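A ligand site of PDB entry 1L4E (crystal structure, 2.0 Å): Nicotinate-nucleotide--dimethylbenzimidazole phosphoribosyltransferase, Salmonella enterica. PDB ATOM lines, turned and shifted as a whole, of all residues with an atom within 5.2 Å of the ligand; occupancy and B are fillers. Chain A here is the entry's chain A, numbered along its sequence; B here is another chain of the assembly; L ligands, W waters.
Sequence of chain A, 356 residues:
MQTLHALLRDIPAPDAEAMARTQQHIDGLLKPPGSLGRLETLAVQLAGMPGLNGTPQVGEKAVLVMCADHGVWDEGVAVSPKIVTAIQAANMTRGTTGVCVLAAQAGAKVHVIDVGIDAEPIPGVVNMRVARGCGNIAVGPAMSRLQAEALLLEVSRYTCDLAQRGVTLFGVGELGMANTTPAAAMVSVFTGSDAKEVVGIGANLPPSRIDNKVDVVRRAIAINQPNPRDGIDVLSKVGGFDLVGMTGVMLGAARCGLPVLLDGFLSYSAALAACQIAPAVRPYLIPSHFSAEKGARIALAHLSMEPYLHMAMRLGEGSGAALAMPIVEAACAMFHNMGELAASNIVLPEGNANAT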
ATOM      1  N   VAL A  77       6.376  11.923  30.879  1.00  0.00           N
ATOM      2  CA  VAL A  77       7.698  12.464  30.592  1.00  0.00           C
ATOM      3  C   VAL A  77       7.996  12.703  29.099  1.00  0.00           C
ATOM      4  O   VAL A  77       9.101  13.133  28.747  1.00  0.00           O
ATOM      5  CB  VAL A  77       8.823  11.555  31.165  1.00  0.00           C
ATOM      6  CG1 VAL A  77       8.699  11.477  32.665  1.00  0.00           C
ATOM      7  CG2 VAL A  77       8.737  10.155  30.544  1.00  0.00           C
ATOM      8  N   ALA A  78       7.012  12.440  28.251  1.00  0.00           N
ATOM      9  CA  ALA A  78       7.176  12.603  26.800  1.00  0.00           C
ATOM     10  C   ALA A  78       5.913  13.183  26.171  1.00  0.00           C
ATOM     11  O   ALA A  78       4.803  12.718  26.439  1.00  0.00           O
ATOM     12  CB  ALA A  78       7.482  11.259  26.156  1.00  0.00           C
ATOM     13  N   SER A  80       5.343  13.258  22.856  1.00  0.00           N
ATOM     14  CA  SER A  80       4.969  12.499  21.663  1.00  0.00           C
ATOM     15  C   SER A  80       4.123  11.265  22.034  1.00  0.00           C
ATOM     16  O   SER A  80       4.414  10.562  22.992  1.00  0.00           O
ATOM     17  CB  SER A  80       6.232  12.052  20.920  1.00  0.00           C
ATOM     18  OG  SER A  80       7.247  13.062  20.956  1.00  0.00           O
ATOM     19  N   VAL A  84       4.015   6.746  18.023  1.00  0.00           N
ATOM     20  CA  VAL A  84       5.019   7.309  17.142  1.00  0.00           C
ATOM     21  C   VAL A  84       6.208   6.340  17.017  1.00  0.00           C
ATOM     22  O   VAL A  84       6.860   6.318  15.982  1.00  0.00           O
ATOM     23  CB  VAL A  84       5.498   8.700  17.660  1.00  0.00           C
ATOM     24  CG1 VAL A  84       6.697   9.193  16.848  1.00  0.00           C
ATOM     25  CG2 VAL A  84       4.359   9.696  17.587  1.00  0.00           C
ATOM     26  N   GLN A  88       7.284   5.441  13.275  1.00  0.00           N
ATOM     27  CA  GLN A  88       8.626   5.791  12.815  1.00  0.00           C
ATOM     28  C   GLN A  88       9.407   4.529  12.457  1.00  0.00           C
ATOM     29  O   GLN A  88      10.238   4.536  11.529  1.00  0.00           O
ATOM     30  CB  GLN A  88       9.394   6.563  13.880  1.00  0.00           C
ATOM     31  CG  GLN A  88       9.325   8.054  13.772  1.00  0.00           C
ATOM     32  CD  GLN A  88       9.826   8.568  12.438  1.00  0.00           C
ATOM     33  OE1 GLN A  88       9.131   8.466  11.427  1.00  0.00           O
ATOM     34  NE2 GLN A  88      11.041   9.125  12.438  1.00  0.00           N
ATOM     35  N   GLU A 174      18.744   4.581  18.036  1.00  0.00           N
ATOM     36  CA  GLU A 174      17.567   4.139  18.757  1.00  0.00           C
ATOM     37  C   GLU A 174      16.302   4.870  18.344  1.00  0.00           C
ATOM     38  O   GLU A 174      16.338   5.869  17.630  1.00  0.00           O
ATOM     39  CB  GLU A 174      17.767   4.284  20.276  1.00  0.00           C
ATOM     40  CG  GLU A 174      18.340   5.648  20.736  1.00  0.00           C
ATOM     41  CD  GLU A 174      17.540   6.834  20.219  1.00  0.00           C
ATOM     42  OE1 GLU A 174      16.338   6.922  20.519  1.00  0.00           O
ATOM     43  OE2 GLU A 174      18.103   7.659  19.500  1.00  0.00           O
ATOM     44  N   LEU A 175      15.178   4.321  18.792  1.00  0.00           N
ATOM     45  CA  LEU A 175      13.865   4.870  18.527  1.00  0.00           C
ATOM     46  C   LEU A 175      12.940   4.390  19.651  1.00  0.00           C
ATOM     47  O   LEU A 175      12.697   3.196  19.787  1.00  0.00           O
ATOM     48  CB  LEU A 175      13.355   4.383  17.174  1.00  0.00           C
ATOM     49  CG  LEU A 175      12.158   5.079  16.550  1.00  0.00           C
ATOM     50  CD1 LEU A 175      12.515   6.566  16.307  1.00  0.00           C
ATOM     51  CD2 LEU A 175      11.793   4.381  15.226  1.00  0.00           C
ATOM     52  N   GLY A 176      12.429   5.313  20.455  1.00  0.00           N
ATOM     53  CA  GLY A 176      11.530   4.917  21.526  1.00  0.00           C
ATOM     54  C   GLY A 176      11.037   6.120  22.293  1.00  0.00           C
ATOM     55  O   GLY A 176      11.821   6.807  22.950  1.00  0.00           O
ATOM     56  N   MET A 177       9.728   6.379  22.231  1.00  0.00           N
ATOM     57  CA  MET A 177       9.170   7.524  22.949  1.00  0.00           C
ATOM     58  C   MET A 177       9.458   7.356  24.448  1.00  0.00           C
ATOM     59  O   MET A 177       9.314   6.267  25.010  1.00  0.00           O
ATOM     60  CB  MET A 177       7.660   7.656  22.712  1.00  0.00           C
ATOM     61  CG  MET A 177       7.264   7.902  21.243  1.00  0.00           C
ATOM     62  SD  MET A 177       8.182   9.245  20.401  1.00  0.00           S
ATOM     63  CE  MET A 177       9.329   8.344  19.484  1.00  0.00           C
ATOM     64  N   ALA A 178       9.901   8.452  25.049  1.00  0.00           N
ATOM     65  CA  ALA A 178      10.252   8.542  26.471  1.00  0.00           C
ATOM     66  C   ALA A 178      11.634   7.988  26.798  1.00  0.00           C
ATOM     67  O   ALA A 178      12.015   7.968  27.975  1.00  0.00           O
ATOM     68  CB  ALA A 178       9.196   7.843  27.345  1.00  0.00           C
ATOM     69  N   ASN A 179      12.425   7.565  25.811  1.00  0.00           N
ATOM     70  CA  ASN A 179      13.710   6.992  26.200  1.00  0.00           C
ATOM     71  C   ASN A 179      14.779   7.937  26.743  1.00  0.00           C
ATOM     72  O   ASN A 179      15.793   7.457  27.237  1.00  0.00           O
ATOM     73  CB  ASN A 179      14.285   6.058  25.100  1.00  0.00           C
ATOM     74  CG  ASN A 179      14.786   6.787  23.863  1.00  0.00           C
ATOM     75  OD1 ASN A 179      14.865   8.001  23.834  1.00  0.00           O
ATOM     76  ND2 ASN A 179      15.146   6.005  22.837  1.00  0.00           N
ATOM     77  N   THR A 180      14.573   9.250  26.726  1.00  0.00           N
ATOM     78  CA  THR A 180      15.608  10.113  27.288  1.00  0.00           C
ATOM     79  C   THR A 180      15.488  10.104  28.805  1.00  0.00           C
ATOM     80  O   THR A 180      16.376  10.596  29.501  1.00  0.00           O
ATOM     81  CB  THR A 180      15.556  11.601  26.747  1.00  0.00           C
ATOM     82  OG1 THR A 180      14.325  12.229  27.111  1.00  0.00           O
ATOM     83  CG2 THR A 180      15.703  11.628  25.226  1.00  0.00           C
ATOM     84  N   THR A 181      14.407   9.523  29.323  1.00  0.00           N
ATOM     85  CA  THR A 181      14.251   9.429  30.768  1.00  0.00           C
ATOM     86  C   THR A 181      15.162   8.330  31.322  1.00  0.00           C
ATOM     87  O   THR A 181      16.007   8.610  32.170  1.00  0.00           O
ATOM     88  CB  THR A 181      12.776   9.228  31.162  1.00  0.00           C
ATOM     89  OG1 THR A 181      12.057  10.420  30.851  1.00  0.00           O
ATOM     90  CG2 THR A 181      12.638   8.984  32.667  1.00  0.00           C
ATOM     91  N   ILE A 201      15.410  18.125  27.614  1.00  0.00           N
ATOM     92  CA  ILE A 201      14.058  18.307  27.078  1.00  0.00           C
ATOM     93  C   ILE A 201      13.627  17.204  26.106  1.00  0.00           C
ATOM     94  O   ILE A 201      12.492  17.183  25.642  1.00  0.00           O
ATOM     95  CB  ILE A 201      13.947  19.677  26.393  1.00  0.00           C
ATOM     96  N   GLY A 202      14.551  16.289  25.792  1.00  0.00           N
ATOM     97  CA  GLY A 202      14.215  15.207  24.875  1.00  0.00           C
ATOM     98  C   GLY A 202      13.541  15.739  23.610  1.00  0.00           C
ATOM     99  O   GLY A 202      13.999  16.721  23.026  1.00  0.00           O
ATOM    100  N   ALA A 203      12.463  15.098  23.182  1.00  0.00           N
ATOM    101  CA  ALA A 203      11.760  15.526  21.981  1.00  0.00           C
ATOM    102  C   ALA A 203      10.836  16.700  22.297  1.00  0.00           C
ATOM    103  O   ALA A 203       9.621  16.558  22.394  1.00  0.00           O
ATOM    104  CB  ALA A 203      10.946  14.350  21.391  1.00  0.00           C
ATOM    105  N   LYS A 213       9.902  15.425  35.179  1.00  0.00           N
ATOM    106  CA  LYS A 213      10.845  14.466  34.619  1.00  0.00           C
ATOM    107  C   LYS A 213      11.968  14.193  35.594  1.00  0.00           C
ATOM    108  O   LYS A 213      12.345  13.046  35.781  1.00  0.00           O
ATOM    109  CB  LYS A 213      11.407  14.999  33.288  1.00  0.00           C
ATOM    110  CG  LYS A 213      12.160  13.975  32.470  1.00  0.00           C
ATOM    111  CD  LYS A 213      12.366  14.504  31.045  1.00  0.00           C
ATOM    112  CE  LYS A 213      13.252  13.588  30.201  1.00  0.00           C
ATOM    113  NZ  LYS A 213      13.440  14.193  28.840  1.00  0.00           N
ATOM    114  N   LEU A 315      18.243  14.696  17.376  1.00  0.00           N
ATOM    115  CA  LEU A 315      17.206  13.858  16.776  1.00  0.00           C
ATOM    116  C   LEU A 315      17.291  12.414  17.228  1.00  0.00           C
ATOM    117  O   LEU A 315      16.274  11.789  17.517  1.00  0.00           O
ATOM    118  CB  LEU A 315      17.284  13.905  15.243  1.00  0.00           C
ATOM    119  CG  LEU A 315      16.450  12.875  14.455  1.00  0.00           C
ATOM    120  CD1 LEU A 315      14.946  13.079  14.747  1.00  0.00           C
ATOM    121  CD2 LEU A 315      16.701  13.042  12.941  1.00  0.00           C
ATOM    122  N   GLY A 316      18.502  11.875  17.305  1.00  0.00           N
ATOM    123  CA  GLY A 316      18.654  10.481  17.682  1.00  0.00           C
ATOM    124  C   GLY A 316      18.567   9.636  16.412  1.00  0.00           C
ATOM    125  O   GLY A 316      18.882  10.129  15.319  1.00  0.00           O
ATOM    126  N   GLU A 317      18.147   8.381  16.553  1.00  0.00           N
ATOM    127  CA  GLU A 317      18.006   7.445  15.427  1.00  0.00           C
ATOM    128  C   GLU A 317      19.319   6.933  14.842  1.00  0.00           C
ATOM    129  O   GLU A 317      19.325   6.038  13.996  1.00  0.00           O
ATOM    130  CB  GLU A 317      17.228   8.089  14.277  1.00  0.00           C
ATOM    131  CG  GLU A 317      15.803   8.461  14.575  1.00  0.00           C
ATOM    132  CD  GLU A 317      15.131   9.085  13.373  1.00  0.00           C
ATOM    133  OE1 GLU A 317      15.675   8.966  12.260  1.00  0.00           O
ATOM    134  OE2 GLU A 317      14.053   9.688  13.541  1.00  0.00           O
ATOM    135  N   LEU B  30       9.728  14.799   9.093  1.00  0.00           N
ATOM    136  CA  LEU B  30       9.550  13.719  10.063  1.00  0.00           C
ATOM    137  C   LEU B  30      10.535  13.754  11.230  1.00  0.00           C
ATOM    138  O   LEU B  30      11.449  12.926  11.346  1.00  0.00           O
ATOM    139  CB  LEU B  30       9.671  12.377   9.306  1.00  0.00           C
ATOM    140  CG  LEU B  30       8.773  11.196   9.630  1.00  0.00           C
ATOM    141  CD1 LEU B  30       7.309  11.605   9.669  1.00  0.00           C
ATOM    142  CD2 LEU B  30       9.005  10.106   8.558  1.00  0.00           C
ATOM    143  N   LYS B  31      10.335  14.700  12.124  1.00  0.00           N
ATOM    144  CA  LYS B  31      11.238  14.852  13.248  1.00  0.00           C
ATOM    145  C   LYS B  31      10.724  15.941  14.143  1.00  0.00           C
ATOM    146  O   LYS B  31       9.946  16.793  13.712  1.00  0.00           O
ATOM    147  CB  LYS B  31      12.619  15.284  12.746  1.00  0.00           C
ATOM    148  CG  LYS B  31      12.541  16.537  11.867  1.00  0.00           C
ATOM    149  CD  LYS B  31      13.912  17.178  11.630  1.00  0.00           C
ATOM    150  CE  LYS B  31      13.797  18.425  10.761  1.00  0.00           C
ATOM    151  NZ  LYS B  31      13.015  19.508  11.421  1.00  0.00           N
ATOM    152  N   PRO B  32      11.136  15.933  15.413  1.00  0.00           N
ATOM    153  CA  PRO B  32      10.632  17.008  16.257  1.00  0.00           C
ATOM    154  C   PRO B  32      11.245  18.299  15.703  1.00  0.00           C
ATOM    155  O   PRO B  32      12.414  18.307  15.293  1.00  0.00           O
ATOM    156  CB  PRO B  32      11.145  16.644  17.660  1.00  0.00           C
ATOM    157  CG  PRO B  32      12.118  15.513  17.440  1.00  0.00           C
ATOM    158  CD  PRO B  32      11.698  14.831  16.199  1.00  0.00           C
ATOM    159  N   LEU B 341       5.681  14.795   8.468  1.00  0.00           N
ATOM    160  CA  LEU B 341       4.843  14.425   9.596  1.00  0.00           C
ATOM    161  C   LEU B 341       3.377  14.183   9.208  1.00  0.00           C
ATOM    162  O   LEU B 341       2.796  13.142   9.553  1.00  0.00           O
ATOM    163  CB  LEU B 341       4.909  15.501  10.676  1.00  0.00           C
ATOM    164  CG  LEU B 341       6.215  15.636  11.479  1.00  0.00           C
ATOM    165  CD1 LEU B 341       6.293  17.022  12.144  1.00  0.00           C
ATOM    166  CD2 LEU B 341       6.292  14.523  12.533  1.00  0.00           C
ATOM    167  N   ILE B 346       1.345  12.231  12.048  1.00  0.00           N
ATOM    168  CA  ILE B 346       1.974  12.554  13.313  1.00  0.00           C
ATOM    169  C   ILE B 346       1.833  14.035  13.619  1.00  0.00           C
ATOM    170  O   ILE B 346       2.166  14.882  12.784  1.00  0.00           O
ATOM    171  CB  ILE B 346       3.465  12.174  13.313  1.00  0.00           C
ATOM    172  CG1 ILE B 346       3.630  10.696  12.978  1.00  0.00           C
ATOM    173  CG2 ILE B 346       4.079  12.469  14.667  1.00  0.00           C
ATOM    174  CD1 ILE B 346       5.071  10.296  12.728  1.00  0.00           C
ATOM    175  N   LEU B 348       2.728  17.056  16.475  1.00  0.00           N
ATOM    176  CA  LEU B 348       3.535  17.410  17.636  1.00  0.00           C
ATOM    177  C   LEU B 348       3.380  18.889  17.968  1.00  0.00           C
ATOM    178  O   LEU B 348       3.395  19.740  17.075  1.00  0.00           O
ATOM    179  CB  LEU B 348       5.005  17.105  17.350  1.00  0.00           C
ATOM    180  CG  LEU B 348       5.313  15.713  16.768  1.00  0.00           C
ATOM    181  CD1 LEU B 348       6.761  15.677  16.317  1.00  0.00           C
ATOM    182  CD2 LEU B 348       5.035  14.636  17.799  1.00  0.00           C
HETATM  183  N1  LIG L   1      13.190  10.340  15.807  1.00  0.00           N
HETATM  184  N2  LIG L   1      13.232  10.667  18.061  1.00  0.00           N
HETATM  185  C1  LIG L   1      13.878  10.239  16.948  1.00  0.00           C
HETATM  186  C2  LIG L   1      11.970  11.082  17.539  1.00  0.00           C
HETATM  187  C3  LIG L   1      11.958  10.873  16.146  1.00  0.00           C
HETATM  188  C4  LIG L   1      10.817  11.210  15.347  1.00  0.00           C
HETATM  189  C5  LIG L   1       9.665  11.759  15.978  1.00  0.00           C
HETATM  190  C6  LIG L   1       9.659  11.967  17.422  1.00  0.00           C
HETATM  191  C7  LIG L   1      10.801  11.633  18.184  1.00  0.00           C
HETATM  192  C8  LIG L   1       8.452  12.124  15.116  1.00  0.00           C
HETATM  193  C9  LIG L   1       8.438  12.547  18.129  1.00  0.00           C
HETATM  194  P1  LIG L   1      11.613  11.678  24.507  1.00  0.00           P
HETATM  195  O1  LIG L   1      12.250  11.040  25.723  1.00  0.00           O
HETATM  196  O2  LIG L   1      11.301  13.103  24.802  1.00  0.00           O
HETATM  197  O3  LIG L   1      10.359  10.974  24.167  1.00  0.00           O
HETATM  198  O4  LIG L   1      12.623  11.617  23.288  1.00  0.00           O
HETATM  199  C10 LIG L   1      13.114  10.345  22.806  1.00  0.00           C
HETATM  200  C11 LIG L   1      12.520   9.930  21.459  1.00  0.00           C
HETATM  201  O5  LIG L   1      12.644  10.982  20.421  1.00  0.00           O
HETATM  202  C12 LIG L   1      13.150   8.740  20.791  1.00  0.00           C
HETATM  203  O6  LIG L   1      12.221   8.050  19.926  1.00  0.00           O
HETATM  204  C13 LIG L   1      14.308   9.414  20.055  1.00  0.00           C
HETATM  205  O7  LIG L   1      14.799   8.509  19.057  1.00  0.00           O
HETATM  206  C14 LIG L   1      13.700  10.709  19.504  1.00  0.00           C
HETATM  207  O   HOH W   1      11.122  14.408  27.387  1.00  0.00           O
HETATM  208  O   HOH W   2       8.997  14.749  24.616  1.00  0.00           O
HETATM  209  O   HOH W   3      11.362  11.248  28.355  1.00  0.00           O
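An oxygen (O6) of the ligand lies close to the backbone carbonyl oxygen (O) of Gly 176 (3.3 Å).
The backbone NH (N) of Thr 180 is in hydrogen-bond range of an oxygen (O1) of the ligand, at 3.1 Å.
N of Ala 178 lies within hydrogen-bond range of O3 of the ligand (2.7 Å).
The side-chain carboxylate (OE1) of Glu 174 is in hydrogen-bond range of an oxygen (O7) of the ligand (2.7 Å).
The backbone NH of Gly 176 sits at hydrogen-bond distance from an oxygen (O6) of the ligand, at 2.8 Å.
An oxygen (O1) of the ligand lies within hydrogen-bond range of the backbone NH (N) of Asn 179.
An oxygen (O2) of the ligand sits at hydrogen-bond distance from the backbone NH (N) of Ala 203 (2.8 Å).
OE2 of Glu 317 sits at hydrogen-bond distance from N1 of the ligand, 2.5 Å away.
The backbone carbonyl oxygen of Glu 174 is in hydrogen-bond range of an oxygen (O7) of the ligand (3.4 Å).
OG1 of Thr 180 sits at hydrogen-bond distance from O1 of the ligand (2.8 Å).
A nitrogen (N2) of the ligand lies close to the backbone carbonyl oxygen (O) of Leu 315 (3.3 Å).
Ala 78 touches the ligand.
Ser 80 touches the ligand.
Val 84 touches the ligand (CG1 to C8, 3.8 Å).
Gln 88 touches the ligand.
Leu 175 touches the ligand (C to O6, 3.7 Å).
Met 177 touches the ligand (CE to O6, 2.9 Å).
CA of Gly 202 touches O2 of the ligand (3.6 Å).
Pro 32 of chain B touches the ligand (CD to C5, 3.7 Å).
Leu 348 of chain B touches the ligand (CD1 to C9, 3.99 Å).
Hydrophobic or aromatic side chains within 4 Å of the ligand: Ala 78, Val 84, Leu 175, Met 177, Ala 203, Leu 315, Pro 32 of chain B and Leu 348 of chain B.
The nearest printed residue that does not touch the ligand is Leu 341 of chain B (4.1 Å).
Water W3 lies within hydrogen-bond range of OG1 of Thr 181 (2.7 Å), O1 of the ligand (2.8 Å), O of Val 77 (3.0 Å), OG1 of Thr 180 (3.4 Å) and O of Ala 178 (3.4 Å).
Water W2 bridges O2 of the ligand and O of Ala 203.
Water W1 lies within hydrogen-bond range of NZ of Lys 213 (2.7 Å), O of Val 77 (2.7 Å) and O2 of the ligand (2.9 Å).
The side-chain amino group (NZ) of Lys 213 is in hydrogen-bond range of the side-chain hydroxyl (OG1) of Thr 180 (2.8 Å).
The backbone carbonyl oxygen (O) of Gly 176 sits close to the side-chain amide oxygen (OD1) of Asn 179 (3.4 Å).
OE1 of Glu 174 lies within hydrogen-bond range of ND2 of Asn 179.
NE2 of Gln 88 is in hydrogen-bond range of OE2 of Glu 317 (3.3 Å).
N of Glu 317 is in hydrogen-bond range of OE2 of Glu 174, at 3.0 Å.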
